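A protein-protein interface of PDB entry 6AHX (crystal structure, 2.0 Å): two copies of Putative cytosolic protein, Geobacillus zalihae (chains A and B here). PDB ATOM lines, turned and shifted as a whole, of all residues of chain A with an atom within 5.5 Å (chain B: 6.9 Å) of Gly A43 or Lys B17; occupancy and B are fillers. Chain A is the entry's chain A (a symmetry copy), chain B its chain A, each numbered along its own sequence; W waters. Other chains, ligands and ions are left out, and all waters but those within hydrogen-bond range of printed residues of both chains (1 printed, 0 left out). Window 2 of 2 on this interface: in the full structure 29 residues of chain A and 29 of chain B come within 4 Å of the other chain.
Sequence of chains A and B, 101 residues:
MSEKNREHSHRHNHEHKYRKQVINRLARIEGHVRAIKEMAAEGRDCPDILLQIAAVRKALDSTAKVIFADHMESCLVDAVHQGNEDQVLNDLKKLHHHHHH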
ATOM      1  N   GLU A  38      10.123  13.967  17.950  1.00  0.00           N
ATOM      2  CA  GLU A  38      10.076  13.315  16.688  1.00  0.00           C
ATOM      3  C   GLU A  38      11.278  12.450  16.522  1.00  0.00           C
ATOM      4  O   GLU A  38      11.162  11.413  15.938  1.00  0.00           O
ATOM      5  CB  GLU A  38       9.926  14.303  15.546  1.00  0.00           C
ATOM      6  CG  GLU A  38       8.572  14.991  15.493  1.00  0.00           C
ATOM      7  CD  GLU A  38       8.552  16.279  14.626  1.00  0.00           C
ATOM      8  OE1 GLU A  38       7.450  16.894  14.532  1.00  0.00           O
ATOM      9  OE2 GLU A  38       9.613  16.706  14.042  1.00  0.00           O
ATOM     10  N   MET A  39      12.423  12.830  17.044  1.00  0.00           N
ATOM     11  CA  MET A  39      13.557  11.931  17.036  1.00  0.00           C
ATOM     12  C   MET A  39      13.264  10.629  17.742  1.00  0.00           C
ATOM     13  O   MET A  39      13.626   9.567  17.275  1.00  0.00           O
ATOM     14  CB  MET A  39      14.777  12.579  17.730  1.00  0.00           C
ATOM     15  CG  MET A  39      15.429  13.730  16.947  1.00  0.00           C
ATOM     16  SD  MET A  39      16.726  14.590  17.883  1.00  0.00           S
ATOM     17  CE  MET A  39      18.016  13.378  17.749  1.00  0.00           C
ATOM     18  N   ALA A  40      12.670  10.719  18.919  1.00  0.00           N
ATOM     19  CA  ALA A  40      12.271   9.549  19.684  1.00  0.00           C
ATOM     20  C   ALA A  40      11.260   8.722  18.914  1.00  0.00           C
ATOM     21  O   ALA A  40      11.415   7.533  18.748  1.00  0.00           O
ATOM     22  CB  ALA A  40      11.701   9.950  21.062  1.00  0.00           C
ATOM     23  N   ALA A  41      10.239   9.362  18.401  1.00  0.00           N
ATOM     24  CA  ALA A  41       9.222   8.660  17.615  1.00  0.00           C
ATOM     25  C   ALA A  41       9.779   7.928  16.399  1.00  0.00           C
ATOM     26  O   ALA A  41       9.279   6.892  16.092  1.00  0.00           O
ATOM     27  CB  ALA A  41       8.148   9.612  17.179  1.00  0.00           C
ATOM     28  N   GLU A  42      10.814   8.464  15.753  1.00  0.00           N
ATOM     29  CA  GLU A  42      11.545   7.833  14.636  1.00  0.00           C
ATOM     30  C   GLU A  42      12.663   6.861  15.024  1.00  0.00           C
ATOM     31  O   GLU A  42      13.304   6.287  14.138  1.00  0.00           O
ATOM     32  CB  GLU A  42      12.203   8.884  13.765  1.00  0.00           C
ATOM     33  CG  GLU A  42      11.277   9.926  13.206  1.00  0.00           C
ATOM     34  CD  GLU A  42      12.024  11.139  12.640  1.00  0.00           C
ATOM     35  OE1 GLU A  42      13.259  11.022  12.386  1.00  0.00           O
ATOM     36  OE2 GLU A  42      11.369  12.212  12.455  1.00  0.00           O
ATOM     37  N   GLY A  43      12.928   6.649  16.314  1.00  0.00           N
ATOM     38  CA  GLY A  43      13.914   5.660  16.707  1.00  0.00           C
ATOM     39  C   GLY A  43      15.340   6.079  16.433  1.00  0.00           C
ATOM     40  O   GLY A  43      16.222   5.264  16.249  1.00  0.00           O
ATOM     41  N   ARG A  44      15.592   7.370  16.549  1.00  0.00           N
ATOM     42  CA  ARG A  44      16.947   7.872  16.482  1.00  0.00           C
ATOM     43  C   ARG A  44      17.859   7.291  17.587  1.00  0.00           C
ATOM     44  O   ARG A  44      17.403   6.808  18.632  1.00  0.00           O
ATOM     45  CB  ARG A  44      16.896   9.381  16.557  1.00  0.00           C
ATOM     46  CG  ARG A  44      16.221  10.068  15.362  1.00  0.00           C
ATOM     47  CD  ARG A  44      17.047  10.032  14.045  1.00  0.00           C
ATOM     48  NE  ARG A  44      18.412  10.545  14.235  1.00  0.00           N
ATOM     49  CZ  ARG A  44      18.779  11.829  14.238  1.00  0.00           C
ATOM     50  NH1 ARG A  44      17.943  12.823  13.968  1.00  0.00           N
ATOM     51  NH2 ARG A  44      20.019  12.117  14.543  1.00  0.00           N
ATOM     52  N   ASP A  45      19.154   7.358  17.358  1.00  0.00           N
ATOM     53  CA  ASP A  45      20.120   6.820  18.306  1.00  0.00           C
ATOM     54  C   ASP A  45      20.072   7.623  19.563  1.00  0.00           C
ATOM     55  O   ASP A  45      19.955   8.835  19.527  1.00  0.00           O
ATOM     56  CB  ASP A  45      21.552   6.800  17.775  1.00  0.00           C
ATOM     57  CG  ASP A  45      21.716   5.883  16.540  1.00  0.00           C
ATOM     58  OD1 ASP A  45      20.902   4.927  16.339  1.00  0.00           O
ATOM     59  OD2 ASP A  45      22.675   6.137  15.782  1.00  0.00           O
ATOM     60  N   CYS A  46      20.159   6.907  20.680  1.00  0.00           N
ATOM     61  CA  CYS A  46      20.015   7.485  21.977  1.00  0.00           C
ATOM     62  C   CYS A  46      20.977   8.644  22.244  1.00  0.00           C
ATOM     63  O   CYS A  46      20.567   9.652  22.761  1.00  0.00           O
ATOM     64  CB  CYS A  46      20.172   6.429  23.032  1.00  0.00           C
ATOM     65  SG  CYS A  46      20.420   7.127  24.664  1.00  0.00           S
ATOM     66  N   LYS B  17      11.056   1.116  19.267  1.00  0.00           N
ATOM     67  CA  LYS B  17      12.414   1.400  19.901  1.00  0.00           C
ATOM     68  C   LYS B  17      12.314   2.149  21.222  1.00  0.00           C
ATOM     69  O   LYS B  17      12.839   1.667  22.191  1.00  0.00           O
ATOM     70  CB  LYS B  17      13.364   2.146  18.973  1.00  0.00           C
ATOM     71  CG  LYS B  17      14.730   2.378  19.586  1.00  0.00           C
ATOM     72  CD  LYS B  17      15.816   2.491  18.520  1.00  0.00           C
ATOM     73  CE  LYS B  17      16.951   3.405  18.968  1.00  0.00           C
ATOM     74  NZ  LYS B  17      17.847   2.938  20.071  1.00  0.00           N
ATOM     75  N   TYR B  18      11.658   3.309  21.280  1.00  0.00           N
ATOM     76  CA  TYR B  18      11.465   3.999  22.579  1.00  0.00           C
ATOM     77  C   TYR B  18      10.088   3.716  23.094  1.00  0.00           C
ATOM     78  O   TYR B  18       9.121   3.717  22.328  1.00  0.00           O
ATOM     79  CB  TYR B  18      11.724   5.529  22.482  1.00  0.00           C
ATOM     80  CG  TYR B  18      13.158   5.807  22.146  1.00  0.00           C
ATOM     81  CD1 TYR B  18      14.133   5.701  23.097  1.00  0.00           C
ATOM     82  CD2 TYR B  18      13.542   6.107  20.861  1.00  0.00           C
ATOM     83  CE1 TYR B  18      15.453   5.933  22.779  1.00  0.00           C
ATOM     84  CE2 TYR B  18      14.866   6.337  20.518  1.00  0.00           C
ATOM     85  CZ  TYR B  18      15.809   6.235  21.468  1.00  0.00           C
ATOM     86  OH  TYR B  18      17.108   6.407  21.144  1.00  0.00           O
ATOM     87  N   ARG B  19       9.965   3.509  24.395  1.00  0.00           N
ATOM     88  CA  ARG B  19       8.634   3.307  24.952  1.00  0.00           C
ATOM     89  C   ARG B  19       7.739   4.498  24.698  1.00  0.00           C
ATOM     90  O   ARG B  19       8.188   5.653  24.722  1.00  0.00           O
ATOM     91  CB  ARG B  19       8.695   2.964  26.422  1.00  0.00           C
ATOM     92  CG  ARG B  19       9.137   1.499  26.619  1.00  0.00           C
ATOM     93  CD  ARG B  19       9.223   1.027  28.078  1.00  0.00           C
ATOM     94  NE  ARG B  19      10.031   1.946  28.895  1.00  0.00           N
ATOM     95  CZ  ARG B  19       9.576   2.977  29.611  1.00  0.00           C
ATOM     96  NH1 ARG B  19       8.274   3.250  29.678  1.00  0.00           N
ATOM     97  NH2 ARG B  19      10.439   3.744  30.282  1.00  0.00           N
ATOM     98  N   ILE B  23       7.941   8.996  24.465  1.00  0.00           N
ATOM     99  CA  ILE B  23       7.466   9.880  23.437  1.00  0.00           C
ATOM    100  C   ILE B  23       6.424  10.849  24.008  1.00  0.00           C
ATOM    101  O   ILE B  23       6.445  12.083  23.732  1.00  0.00           O
ATOM    102  CB  ILE B  23       6.962   9.072  22.201  1.00  0.00           C
ATOM    103  CG1 ILE B  23       8.161   8.463  21.443  1.00  0.00           C
ATOM    104  CG2 ILE B  23       6.258   9.981  21.194  1.00  0.00           C
ATOM    105  CD1 ILE B  23       8.312   6.976  21.533  1.00  0.00           C
ATOM    106  N   ASP B  70      16.538   2.626  29.904  1.00  0.00           N
ATOM    107  CA  ASP B  70      16.046   1.736  28.852  1.00  0.00           C
ATOM    108  C   ASP B  70      17.011   1.318  27.739  1.00  0.00           C
ATOM    109  O   ASP B  70      16.817   0.276  27.138  1.00  0.00           O
ATOM    110  CB  ASP B  70      14.851   2.375  28.167  1.00  0.00           C
ATOM    111  CG  ASP B  70      13.670   2.530  29.067  1.00  0.00           C
ATOM    112  OD1 ASP B  70      13.736   2.100  30.227  1.00  0.00           O
ATOM    113  OD2 ASP B  70      12.670   3.138  28.576  1.00  0.00           O
ATOM    114  N   HIS B  71      17.985   2.163  27.408  1.00  0.00           N
ATOM    115  CA  HIS B  71      18.849   1.973  26.254  1.00  0.00           C
ATOM    116  C   HIS B  71      20.297   2.122  26.638  1.00  0.00           C
ATOM    117  O   HIS B  71      21.107   2.494  25.830  1.00  0.00           O
ATOM    118  CB  HIS B  71      18.450   2.953  25.128  1.00  0.00           C
ATOM    119  CG  HIS B  71      17.024   2.796  24.703  1.00  0.00           C
ATOM    120  ND1 HIS B  71      16.631   1.832  23.802  1.00  0.00           N
ATOM    121  CD2 HIS B  71      15.883   3.399  25.127  1.00  0.00           C
ATOM    122  CE1 HIS B  71      15.313   1.845  23.678  1.00  0.00           C
ATOM    123  NE2 HIS B  71      14.832   2.776  24.484  1.00  0.00           N
ATOM    124  N   SER B  74      23.368   1.264  24.219  1.00  0.00           N
ATOM    125  CA  SER B  74      23.506   2.188  23.085  1.00  0.00           C
ATOM    126  C   SER B  74      23.639   3.668  23.458  1.00  0.00           C
ATOM    127  O   SER B  74      24.167   4.410  22.681  1.00  0.00           O
ATOM    128  CB  SER B  74      22.347   1.996  22.102  1.00  0.00           C
ATOM    129  OG  SER B  74      21.173   2.450  22.688  1.00  0.00           O
HETATM  130  O   HOH W   1      10.768   4.832  18.930  1.00  0.00           O
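The backbone carbonyl oxygen (O) of Lys B17 sits close to a ring nitrogen (NE2) of His B71 (3.2 Å).
O of Met A39 sits at hydrogen-bond distance from N of Arg A44 (3.0 Å).
Printed residues of chain A that touch a printed residue of chain B: Ala A40, Ala A41, Gly A43, Arg A44, Asp A45 and Cys A46.
Among the printed residues, 9 pairs touch across the chains.
Among the printed residues, no Asp or Glu carboxylate lies within 4 Å of a Lys or Arg side-chain nitrogen of the other chain.
Water W1 bridges O of Ala A40 and N of Tyr B18.
Lys B17 touches just these residues of chain A: Gly A43 (3.4 Å) and Arg A44 (3.4 Å).
Of the printed residues of chain B, Ala A41 touches Ile B23 (3.8 Å).
Of the printed residues of chain A, Ile B23 touches Ala A40 and Ala A41.
Printed residues of chain B within 4 Å of Arg A44: Lys B17 and Tyr B18.
Of the printed residues of chain B, Cys A46 touches Tyr B18 (3.1 Å).
Printed residues of chain A within 4 Å of Tyr B18: Ala A40 (3.3 Å), Gly A43 (3.99 Å), Arg A44 (2.6 Å), Asp A45 (3.6 Å) and Cys A46 (3.1 Å).
OH of Tyr B18 sits at hydrogen-bond distance from O of Arg A44 (2.6 Å).
The backbone NH (N) of Cys A46 sits at hydrogen-bond distance from the side-chain hydroxyl (OH) of Tyr B18 (3.1 Å).
Among the printed residues, pairs that only touch across the chains: Ala A40 with Tyr B18, Gly A43 with Lys B17, Arg A44 with Lys B17, Asp A45 with Tyr B18, Ala A41 with Ile B23, Ala A40 with Ile B23 and Gly A43 with Tyr B18.
No position is printed for both chains.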
